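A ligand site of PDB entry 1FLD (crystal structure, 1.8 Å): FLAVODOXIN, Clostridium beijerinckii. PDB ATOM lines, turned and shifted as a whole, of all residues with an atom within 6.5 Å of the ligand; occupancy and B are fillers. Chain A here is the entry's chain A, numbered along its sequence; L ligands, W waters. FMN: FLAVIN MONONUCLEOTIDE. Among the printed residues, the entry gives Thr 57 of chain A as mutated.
The backbone NH (N) of Thr 9 is in hydrogen-bond range of an oxygen (O1P) of the ligand (2.7 Å). An oxygen (O1P) of the ligand sits at hydrogen-bond distance from the side-chain hydroxyl (OG1) of Thr 9 (2.6 Å). The side-chain hydroxyl (OG) of Ser 7 is in hydrogen-bond range of an oxygen (O2P) of the ligand (2.7 Å). The backbone NH (N) of Ala 55 is in hydrogen-bond range of an oxygen (O2') of the ligand (3.3 Å). O2' of the ligand is in hydrogen-bond range of O of Ala 55, 2.7 Å away. N of Asn 11 sits at hydrogen-bond distance from O1P of the ligand (3.1 Å). The side-chain amide oxygen (OD1) of Asn 11 sits at hydrogen-bond distance from an oxygen (O4') of the ligand (2.8 Å). N of Gly 91 lies within hydrogen-bond range of O2 of the ligand (2.8 Å). The backbone NH (N) of Thr 12 lies within hydrogen-bond range of an oxygen (O2P) of the ligand (2.8 Å). O2P of the ligand lies within hydrogen-bond range of OG1 of Thr 12 (2.8 Å). N of Gly 8 lies within hydrogen-bond range of O3P of the ligand (2.8 Å). OG of Ser 54 is in hydrogen-bond range of O3P of the ligand, 2.8 Å away. An oxygen (O4') of the ligand is in hydrogen-bond range of the side-chain hydroxyl of Ser 87 (2.8 Å). An oxygen (O4) of the ligand is in hydrogen-bond range of the backbone NH of Glu 59 (3.1 Å). The side-chain carboxylate of Glu 59 is in hydrogen-bond range of a nitrogen (N3) of the ligand (2.8 Å). O2 of the ligand sits at hydrogen-bond distance from N of Gly 89 (3.0 Å). An oxygen (O1P) of the ligand is in hydrogen-bond range of the backbone NH of Gly 10, 3.0 Å away. The backbone NH (N) of Trp 90 lies within hydrogen-bond range of an oxygen (O2) of the ligand.
The backbone carbonyl oxygen (O) of Met 56 sits close to an oxygen (O4) of the ligand (3.3 Å). Trp 6 touches the ligand (CZ3 to O3P, 3.97 Å). Thr 57 touches the ligand (N to C6, 3.4 Å). Asp 58 touches the ligand (N to O4, 3.6 Å). Tyr 88 touches the ligand (CA to O2', 3.5 Å). Asn 119 touches the ligand. Hydrophobic or aromatic side chains that line the ligand: Trp 6, Ala 55, Met 56, Tyr 88 and Trp 90. Of the 29 residues printed, 19 come within 4 Å of the ligand. The nearest printed residue that does not touch the ligand is Glu 13 (4.5 Å).
Water W5 lies within hydrogen-bond range of the side-chain amide oxygen of Asn 119, an oxygen (O3') of the ligand and the side-chain amide oxygen of Asn 11. Water W3 bridges N of Asp 58 and O4 of the ligand. Water W2 bridges OG1 of Thr 57 (2.8 Å) and SD of Met 56 (2.9 Å). Water W1 lies within hydrogen-bond range of OE1 of Glu 59, N of Gly 93, O2 of the ligand and N of Asp 92.
N of Thr 12 lies within hydrogen-bond range of OG of Ser 7 (3.4 Å). The side-chain hydroxyl of Ser 7 is in hydrogen-bond range of the backbone NH of Gly 10 (3.0 Å). OG of Ser 7 sits at hydrogen-bond distance from N of Glu 13 (3.3 Å). OG of Ser 87 lies within hydrogen-bond range of O of Asn 119 (2.6 Å). OG of Ser 87 lies close to O of Val 117 (3.2 Å). The backbone NH (N) of Ser 87 lies close to the side-chain sulfur (SD) of Met 15 (3.8 Å). The backbone carbonyl oxygen of Gly 89 sits at hydrogen-bond distance from the side-chain amide nitrogen of Gln 118 (2.9 Å). The backbone carbonyl oxygen of Tyr 88 is in hydrogen-bond range of the backbone NH of Asn 119, at 2.8 Å.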
ATOM      1  N   TRP A   6      21.790  12.716   1.590  1.00  0.00           N
ATOM      2  CA  TRP A   6      20.926  13.698   2.246  1.00  0.00           C
ATOM      3  C   TRP A   6      21.181  14.970   1.408  1.00  0.00           C
ATOM      4  O   TRP A   6      22.338  15.275   1.084  1.00  0.00           O
ATOM      5  CB  TRP A   6      21.294  13.983   3.711  1.00  0.00           C
ATOM      6  CG  TRP A   6      20.306  14.984   4.327  1.00  0.00           C
ATOM      7  CD1 TRP A   6      19.092  14.689   4.885  1.00  0.00           C
ATOM      8  CD2 TRP A   6      20.402  16.423   4.316  1.00  0.00           C
ATOM      9  NE1 TRP A   6      18.420  15.852   5.213  1.00  0.00           N
ATOM     10  CE2 TRP A   6      19.201  16.928   4.873  1.00  0.00           C
ATOM     11  CE3 TRP A   6      21.376  17.336   3.893  1.00  0.00           C
ATOM     12  CZ2 TRP A   6      18.953  18.301   5.017  1.00  0.00           C
ATOM     13  CZ3 TRP A   6      21.127  18.709   4.048  1.00  0.00           C
ATOM     14  CH2 TRP A   6      19.919  19.175   4.596  1.00  0.00           C
ATOM     15  N   SER A   7      20.121  15.691   1.050  1.00  0.00           N
ATOM     16  CA  SER A   7      20.261  16.930   0.289  1.00  0.00           C
ATOM     17  C   SER A   7      19.208  17.923   0.784  1.00  0.00           C
ATOM     18  O   SER A   7      18.034  17.565   0.947  1.00  0.00           O
ATOM     19  CB  SER A   7      20.074  16.642  -1.199  1.00  0.00           C
ATOM     20  OG  SER A   7      20.373  17.791  -1.982  1.00  0.00           O
ATOM     21  N   GLY A   8      19.628  19.167   1.047  1.00  0.00           N
ATOM     22  CA  GLY A   8      18.712  20.179   1.562  1.00  0.00           C
ATOM     23  C   GLY A   8      18.075  21.053   0.507  1.00  0.00           C
ATOM     24  O   GLY A   8      17.001  21.600   0.735  1.00  0.00           O
ATOM     25  N   THR A   9      18.749  21.266  -0.623  1.00  0.00           N
ATOM     26  CA  THR A   9      18.181  22.072  -1.694  1.00  0.00           C
ATOM     27  C   THR A   9      18.193  21.328  -3.030  1.00  0.00           C
ATOM     28  O   THR A   9      17.650  21.810  -4.025  1.00  0.00           O
ATOM     29  CB  THR A   9      18.891  23.438  -1.872  1.00  0.00           C
ATOM     30  OG1 THR A   9      20.183  23.249  -2.467  1.00  0.00           O
ATOM     31  CG2 THR A   9      19.040  24.164  -0.531  1.00  0.00           C
ATOM     32  N   GLY A  10      18.841  20.169  -3.079  1.00  0.00           N
ATOM     33  CA  GLY A  10      18.879  19.391  -4.308  1.00  0.00           C
ATOM     34  C   GLY A  10      20.233  19.278  -4.980  1.00  0.00           C
ATOM     35  O   GLY A  10      20.357  18.578  -5.979  1.00  0.00           O
ATOM     36  N   ASN A  11      21.261  19.939  -4.445  1.00  0.00           N
ATOM     37  CA  ASN A  11      22.574  19.869  -5.056  1.00  0.00           C
ATOM     38  C   ASN A  11      23.206  18.482  -4.960  1.00  0.00           C
ATOM     39  O   ASN A  11      23.637  17.923  -5.982  1.00  0.00           O
ATOM     40  CB  ASN A  11      23.495  20.949  -4.474  1.00  0.00           C
ATOM     41  CG  ASN A  11      23.041  22.336  -4.827  1.00  0.00           C
ATOM     42  OD1 ASN A  11      23.399  23.330  -4.172  1.00  0.00           O
ATOM     43  ND2 ASN A  11      22.229  22.440  -5.877  1.00  0.00           N
ATOM     44  N   THR A  12      23.250  17.932  -3.751  1.00  0.00           N
ATOM     45  CA  THR A  12      23.799  16.590  -3.528  1.00  0.00           C
ATOM     46  C   THR A  12      22.902  15.532  -4.169  1.00  0.00           C
ATOM     47  O   THR A  12      23.404  14.490  -4.612  1.00  0.00           O
ATOM     48  CB  THR A  12      23.992  16.311  -2.011  1.00  0.00           C
ATOM     49  OG1 THR A  12      24.858  17.311  -1.463  1.00  0.00           O
ATOM     50  CG2 THR A  12      24.640  14.945  -1.793  1.00  0.00           C
ATOM     51  N   GLU A  13      21.600  15.786  -4.238  1.00  0.00           N
ATOM     52  CA  GLU A  13      20.662  14.862  -4.873  1.00  0.00           C
ATOM     53  C   GLU A  13      20.962  14.743  -6.361  1.00  0.00           C
ATOM     54  O   GLU A  13      20.922  13.654  -6.932  1.00  0.00           O
ATOM     55  CB  GLU A  13      19.224  15.331  -4.694  1.00  0.00           C
ATOM     56  CG  GLU A  13      18.225  14.351  -5.294  1.00  0.00           C
ATOM     57  CD  GLU A  13      16.787  14.808  -5.194  1.00  0.00           C
ATOM     58  OE1 GLU A  13      16.509  15.995  -4.951  1.00  0.00           O
ATOM     59  OE2 GLU A  13      15.907  13.945  -5.399  1.00  0.00           O
ATOM     60  N   MET A  15      23.869  15.331  -7.730  1.00  0.00           N
ATOM     61  CA  MET A  15      25.139  14.586  -7.855  1.00  0.00           C
ATOM     62  C   MET A  15      24.869  13.088  -7.815  1.00  0.00           C
ATOM     63  O   MET A  15      25.432  12.329  -8.602  1.00  0.00           O
ATOM     64  CB  MET A  15      26.106  14.931  -6.721  1.00  0.00           C
ATOM     65  CG  MET A  15      26.621  16.328  -6.748  1.00  0.00           C
ATOM     66  SD  MET A  15      27.772  16.624  -5.410  1.00  0.00           S
ATOM     67  CE  MET A  15      27.774  18.279  -5.491  1.00  0.00           C
ATOM     68  N   CYS A  53      26.494  13.734   1.311  1.00  0.00           N
ATOM     69  CA  CYS A  53      25.827  14.715   2.159  1.00  0.00           C
ATOM     70  C   CYS A  53      26.520  16.055   1.980  1.00  0.00           C
ATOM     71  O   CYS A  53      27.740  16.114   1.864  1.00  0.00           O
ATOM     72  CB  CYS A  53      25.931  14.293   3.632  1.00  0.00           C
ATOM     73  SG  CYS A  53      25.083  15.409   4.768  1.00  0.00           S
ATOM     74  N   SER A  54      25.737  17.129   1.903  1.00  0.00           N
ATOM     75  CA  SER A  54      26.310  18.467   1.756  1.00  0.00           C
ATOM     76  C   SER A  54      26.945  18.970   3.054  1.00  0.00           C
ATOM     77  O   SER A  54      26.736  18.406   4.134  1.00  0.00           O
ATOM     78  CB  SER A  54      25.217  19.431   1.316  1.00  0.00           C
ATOM     79  OG  SER A  54      24.088  19.289   2.150  1.00  0.00           O
ATOM     80  N   ALA A  55      27.721  20.055   2.945  1.00  0.00           N
ATOM     81  CA  ALA A  55      28.386  20.629   4.100  1.00  0.00           C
ATOM     82  C   ALA A  55      27.409  21.468   4.921  1.00  0.00           C
ATOM     83  O   ALA A  55      26.776  22.368   4.381  1.00  0.00           O
ATOM     84  CB  ALA A  55      29.555  21.473   3.660  1.00  0.00           C
ATOM     85  N   MET A  56      27.239  21.106   6.187  1.00  0.00           N
ATOM     86  CA  MET A  56      26.351  21.844   7.079  1.00  0.00           C
ATOM     87  C   MET A  56      27.126  22.665   8.112  1.00  0.00           C
ATOM     88  O   MET A  56      28.360  22.603   8.179  1.00  0.00           O
ATOM     89  CB  MET A  56      25.317  20.932   7.736  1.00  0.00           C
ATOM     90  CG  MET A  56      24.174  20.513   6.803  1.00  0.00           C
ATOM     91  SD  MET A  56      23.180  21.876   6.087  1.00  0.00           S
ATOM     92  CE  MET A  56      23.691  21.780   4.366  1.00  0.00           C
ATOM     93  N   THR A  57      26.382  23.417   8.913  1.00  0.00           N
ATOM     94  CA  THR A  57      26.915  24.337   9.914  1.00  0.00           C
ATOM     95  C   THR A  57      28.232  23.985  10.570  1.00  0.00           C
ATOM     96  O   THR A  57      28.332  22.973  11.281  1.00  0.00           O
ATOM     97  CB  THR A  57      25.870  24.676  10.992  1.00  0.00           C
ATOM     98  OG1 THR A  57      24.626  25.001  10.359  1.00  0.00           O
ATOM     99  CG2 THR A  57      26.330  25.867  11.822  1.00  0.00           C
ATOM    100  N   ASP A  58      29.215  24.850  10.344  1.00  0.00           N
ATOM    101  CA  ASP A  58      30.558  24.694  10.879  1.00  0.00           C
ATOM    102  C   ASP A  58      31.250  23.458  10.326  1.00  0.00           C
ATOM    103  O   ASP A  58      31.964  22.761  11.046  1.00  0.00           O
ATOM    104  CB  ASP A  58      30.565  24.699  12.420  1.00  0.00           C
ATOM    105  CG  ASP A  58      30.220  26.068  13.017  1.00  0.00           C
ATOM    106  OD1 ASP A  58      30.292  27.088  12.290  1.00  0.00           O
ATOM    107  OD2 ASP A  58      29.879  26.126  14.218  1.00  0.00           O
ATOM    108  N   GLU A  59      31.012  23.188   9.042  1.00  0.00           N
ATOM    109  CA  GLU A  59      31.632  22.069   8.338  1.00  0.00           C
ATOM    110  C   GLU A  59      31.393  20.704   8.951  1.00  0.00           C
ATOM    111  O   GLU A  59      32.342  19.968   9.263  1.00  0.00           O
ATOM    112  CB  GLU A  59      33.153  22.292   8.215  1.00  0.00           C
ATOM    113  CG  GLU A  59      33.574  23.546   7.475  1.00  0.00           C
ATOM    114  CD  GLU A  59      33.329  23.487   5.973  1.00  0.00           C
ATOM    115  OE1 GLU A  59      33.299  22.385   5.383  1.00  0.00           O
ATOM    116  OE2 GLU A  59      33.218  24.567   5.367  1.00  0.00           O
ATOM    117  N   VAL A  60      30.125  20.338   9.100  1.00  0.00           N
ATOM    118  CA  VAL A  60      29.772  19.030   9.662  1.00  0.00           C
ATOM    119  C   VAL A  60      28.758  18.343   8.757  1.00  0.00           C
ATOM    120  O   VAL A  60      28.216  18.962   7.824  1.00  0.00           O
ATOM    121  CB  VAL A  60      29.140  19.156  11.090  1.00  0.00           C
ATOM    122  CG1 VAL A  60      30.102  19.837  12.049  1.00  0.00           C
ATOM    123  CG2 VAL A  60      27.810  19.911  11.023  1.00  0.00           C
ATOM    124  N   SER A  87      27.992  18.210  -1.988  1.00  0.00           N
ATOM    125  CA  SER A  87      28.084  19.584  -2.452  1.00  0.00           C
ATOM    126  C   SER A  87      28.404  20.480  -1.268  1.00  0.00           C
ATOM    127  O   SER A  87      28.028  20.174  -0.128  1.00  0.00           O
ATOM    128  CB  SER A  87      26.743  20.006  -3.055  1.00  0.00           C
ATOM    129  OG  SER A  87      26.826  21.306  -3.636  1.00  0.00           O
ATOM    130  N   TYR A  88      29.040  21.604  -1.543  1.00  0.00           N
ATOM    131  CA  TYR A  88      29.401  22.537  -0.487  1.00  0.00           C
ATOM    132  C   TYR A  88      29.264  23.954  -1.018  1.00  0.00           C
ATOM    133  O   TYR A  88      29.106  24.161  -2.221  1.00  0.00           O
ATOM    134  CB  TYR A  88      30.809  22.261   0.045  1.00  0.00           C
ATOM    135  CG  TYR A  88      31.895  22.543  -0.957  1.00  0.00           C
ATOM    136  CD1 TYR A  88      32.156  21.654  -1.993  1.00  0.00           C
ATOM    137  CD2 TYR A  88      32.678  23.704  -0.867  1.00  0.00           C
ATOM    138  CE1 TYR A  88      33.158  21.897  -2.914  1.00  0.00           C
ATOM    139  CE2 TYR A  88      33.683  23.955  -1.798  1.00  0.00           C
ATOM    140  CZ  TYR A  88      33.914  23.044  -2.807  1.00  0.00           C
ATOM    141  OH  TYR A  88      34.918  23.266  -3.716  1.00  0.00           O
ATOM    142  N   GLY A  89      29.325  24.925  -0.112  1.00  0.00           N
ATOM    143  CA  GLY A  89      29.157  26.292  -0.522  1.00  0.00           C
ATOM    144  C   GLY A  89      30.394  27.145  -0.476  1.00  0.00           C
ATOM    145  O   GLY A  89      31.192  27.138  -1.410  1.00  0.00           O
ATOM    146  N   TRP A  90      30.589  27.822   0.643  1.00  0.00           N
ATOM    147  CA  TRP A  90      31.697  28.752   0.827  1.00  0.00           C
ATOM    148  C   TRP A  90      33.005  28.203   1.383  1.00  0.00           C
ATOM    149  O   TRP A  90      34.020  28.924   1.384  1.00  0.00           O
ATOM    150  CB  TRP A  90      31.226  29.913   1.702  1.00  0.00           C
ATOM    151  CG  TRP A  90      30.640  29.469   3.032  1.00  0.00           C
ATOM    152  CD1 TRP A  90      31.314  29.216   4.194  1.00  0.00           C
ATOM    153  CD2 TRP A  90      29.246  29.241   3.326  1.00  0.00           C
ATOM    154  NE1 TRP A  90      30.432  28.864   5.180  1.00  0.00           N
ATOM    155  CE2 TRP A  90      29.162  28.870   4.686  1.00  0.00           C
ATOM    156  CE3 TRP A  90      28.070  29.329   2.567  1.00  0.00           C
ATOM    157  CZ2 TRP A  90      27.941  28.589   5.303  1.00  0.00           C
ATOM    158  CZ3 TRP A  90      26.855  29.036   3.196  1.00  0.00           C
ATOM    159  CH2 TRP A  90      26.804  28.668   4.551  1.00  0.00           C
ATOM    160  N   GLY A  91      33.006  26.972   1.871  1.00  0.00           N
ATOM    161  CA  GLY A  91      34.211  26.397   2.444  1.00  0.00           C
ATOM    162  C   GLY A  91      35.150  25.818   1.407  1.00  0.00           C
ATOM    163  O   GLY A  91      35.007  26.094   0.212  1.00  0.00           O
ATOM    164  N   ASP A  92      36.090  25.005   1.855  1.00  0.00           N
ATOM    165  CA  ASP A  92      37.048  24.384   0.955  1.00  0.00           C
ATOM    166  C   ASP A  92      37.109  22.860   1.097  1.00  0.00           C
ATOM    167  O   ASP A  92      38.111  22.245   0.760  1.00  0.00           O
ATOM    168  CB  ASP A  92      38.458  24.992   1.114  1.00  0.00           C
ATOM    169  CG  ASP A  92      39.056  24.797   2.504  1.00  0.00           C
ATOM    170  OD1 ASP A  92      38.550  23.977   3.314  1.00  0.00           O
ATOM    171  OD2 ASP A  92      40.064  25.466   2.791  1.00  0.00           O
ATOM    172  N   GLY A  93      36.031  22.284   1.623  1.00  0.00           N
ATOM    173  CA  GLY A  93      35.975  20.839   1.762  1.00  0.00           C
ATOM    174  C   GLY A  93      36.326  20.281   3.119  1.00  0.00           C
ATOM    175  O   GLY A  93      36.464  19.067   3.241  1.00  0.00           O
ATOM    176  N   TRP A  95      34.529  19.666   5.739  1.00  0.00           N
ATOM    177  CA  TRP A  95      33.577  18.645   6.182  1.00  0.00           C
ATOM    178  C   TRP A  95      33.848  17.282   5.534  1.00  0.00           C
ATOM    179  O   TRP A  95      33.674  16.253   6.175  1.00  0.00           O
ATOM    180  CB  TRP A  95      32.118  19.097   5.955  1.00  0.00           C
ATOM    181  CG  TRP A  95      31.414  18.470   4.777  1.00  0.00           C
ATOM    182  CD1 TRP A  95      30.379  17.570   4.825  1.00  0.00           C
ATOM    183  CD2 TRP A  95      31.662  18.717   3.379  1.00  0.00           C
ATOM    184  NE1 TRP A  95      29.969  17.240   3.550  1.00  0.00           N
ATOM    185  CE2 TRP A  95      30.732  17.932   2.644  1.00  0.00           C
ATOM    186  CE3 TRP A  95      32.564  19.526   2.679  1.00  0.00           C
ATOM    187  CZ2 TRP A  95      30.693  17.940   1.250  1.00  0.00           C
ATOM    188  CZ3 TRP A  95      32.527  19.533   1.275  1.00  0.00           C
ATOM    189  CH2 TRP A  95      31.588  18.741   0.580  1.00  0.00           C
ATOM    190  N   VAL A 117      31.678  19.072  -5.032  1.00  0.00           N
ATOM    191  CA  VAL A 117      31.333  20.062  -6.052  1.00  0.00           C
ATOM    192  C   VAL A 117      30.696  21.237  -5.354  1.00  0.00           C
ATOM    193  O   VAL A 117      29.915  21.065  -4.406  1.00  0.00           O
ATOM    194  CB  VAL A 117      30.319  19.464  -7.085  1.00  0.00           C
ATOM    195  CG1 VAL A 117      29.769  20.538  -7.999  1.00  0.00           C
ATOM    196  CG2 VAL A 117      30.979  18.351  -7.895  1.00  0.00           C
ATOM    197  N   GLN A 118      31.081  22.439  -5.763  1.00  0.00           N
ATOM    198  CA  GLN A 118      30.539  23.640  -5.154  1.00  0.00           C
ATOM    199  C   GLN A 118      29.171  23.924  -5.732  1.00  0.00           C
ATOM    200  O   GLN A 118      29.026  24.046  -6.947  1.00  0.00           O
ATOM    201  CB  GLN A 118      31.468  24.816  -5.429  1.00  0.00           C
ATOM    202  CG  GLN A 118      31.024  26.107  -4.781  1.00  0.00           C
ATOM    203  CD  GLN A 118      32.020  27.228  -4.971  1.00  0.00           C
ATOM    204  OE1 GLN A 118      32.714  27.296  -5.987  1.00  0.00           O
ATOM    205  NE2 GLN A 118      32.102  28.114  -3.995  1.00  0.00           N
ATOM    206  N   ASN A 119      28.177  24.029  -4.854  1.00  0.00           N
ATOM    207  CA  ASN A 119      26.797  24.301  -5.250  1.00  0.00           C
ATOM    208  C   ASN A 119      26.263  23.258  -6.232  1.00  0.00           C
ATOM    209  O   ASN A 119      26.612  22.085  -6.132  1.00  0.00           O
ATOM    210  CB  ASN A 119      26.685  25.723  -5.798  1.00  0.00           C
ATOM    211  CG  ASN A 119      27.246  26.769  -4.842  1.00  0.00           C
ATOM    212  OD1 ASN A 119      26.846  26.830  -3.659  1.00  0.00           O
ATOM    213  ND2 ASN A 119      28.207  27.550  -5.308  1.00  0.00           N
ATOM    214  N   GLU A 120      25.423  23.660  -7.185  1.00  0.00           N
ATOM    215  CA  GLU A 120      24.857  22.688  -8.126  1.00  0.00           C
ATOM    216  C   GLU A 120      25.886  22.200  -9.136  1.00  0.00           C
ATOM    217  O   GLU A 120      26.672  22.992  -9.659  1.00  0.00           O
ATOM    218  CB  GLU A 120      23.652  23.289  -8.853  1.00  0.00           C
ATOM    219  CG  GLU A 120      22.786  22.252  -9.581  1.00  0.00           C
ATOM    220  CD  GLU A 120      21.551  22.852 -10.252  1.00  0.00           C
ATOM    221  OE1 GLU A 120      20.809  23.609  -9.582  1.00  0.00           O
ATOM    222  OE2 GLU A 120      21.318  22.532 -11.450  1.00  0.00           O
HETATM  223  N1  FMN L   1      28.880  25.207   2.863  1.00  0.00           N
HETATM  224  C2  FMN L   1      30.184  25.106   3.206  1.00  0.00           C
HETATM  225  O2  FMN L   1      31.041  25.087   2.342  1.00  0.00           O
HETATM  226  N3  FMN L   1      30.538  25.051   4.580  1.00  0.00           N
HETATM  227  C4  FMN L   1      29.665  25.142   5.649  1.00  0.00           C
HETATM  228  O4  FMN L   1      30.049  25.126   6.833  1.00  0.00           O
HETATM  229  C4A FMN L   1      28.247  25.259   5.258  1.00  0.00           C
HETATM  230  N5  FMN L   1      27.336  25.397   6.187  1.00  0.00           N
HETATM  231  C5A FMN L   1      26.036  25.567   5.789  1.00  0.00           C
HETATM  232  C6  FMN L   1      25.029  25.729   6.763  1.00  0.00           C
HETATM  233  C7  FMN L   1      23.709  25.722   6.425  1.00  0.00           C
HETATM  234  C7M FMN L   1      22.647  25.848   7.484  1.00  0.00           C
HETATM  235  C8  FMN L   1      23.327  25.628   5.067  1.00  0.00           C
HETATM  236  C8M FMN L   1      21.889  25.667   4.627  1.00  0.00           C
HETATM  237  C9  FMN L   1      24.297  25.527   4.094  1.00  0.00           C
HETATM  238  C9A FMN L   1      25.648  25.486   4.429  1.00  0.00           C
HETATM  239  N10 FMN L   1      26.649  25.388   3.461  1.00  0.00           N
HETATM  240  C10 FMN L   1      27.962  25.284   3.805  1.00  0.00           C
HETATM  241  C1' FMN L   1      26.275  25.425   2.055  1.00  0.00           C
HETATM  242  C2' FMN L   1      25.831  24.074   1.471  1.00  0.00           C
HETATM  243  O2' FMN L   1      26.764  23.021   1.742  1.00  0.00           O
HETATM  244  C3' FMN L   1      25.666  24.212  -0.042  1.00  0.00           C
HETATM  245  O3' FMN L   1      24.652  25.182  -0.319  1.00  0.00           O
HETATM  246  C4' FMN L   1      25.347  22.917  -0.803  1.00  0.00           C
HETATM  247  O4' FMN L   1      25.321  23.190  -2.204  1.00  0.00           O
HETATM  248  C5' FMN L   1      23.998  22.363  -0.370  1.00  0.00           C
HETATM  249  O5' FMN L   1      23.759  21.155  -1.044  1.00  0.00           O
HETATM  250  P   FMN L   1      22.363  20.429  -0.889  1.00  0.00           P
HETATM  251  O1P FMN L   1      21.295  21.111  -1.570  1.00  0.00           O
HETATM  252  O2P FMN L   1      22.630  19.044  -1.293  1.00  0.00           O
HETATM  253  O3P FMN L   1      22.054  20.426   0.595  1.00  0.00           O
HETATM  254  O   HOH W   1      33.453  22.923   2.645  1.00  0.00           O
HETATM  255  O   HOH W   2      23.485  23.076   8.686  1.00  0.00           O
HETATM  256  O   HOH W   3      28.740  26.961   8.581  1.00  0.00           O
HETATM  257  O   HOH W   4      22.253  24.896   1.186  1.00  0.00           O
HETATM  258  O   HOH W   5      24.476  26.230  -2.787  1.00  0.00           O
HETATM  259  O   HOH W   6      21.113  22.625   2.030  1.00  0.00           O
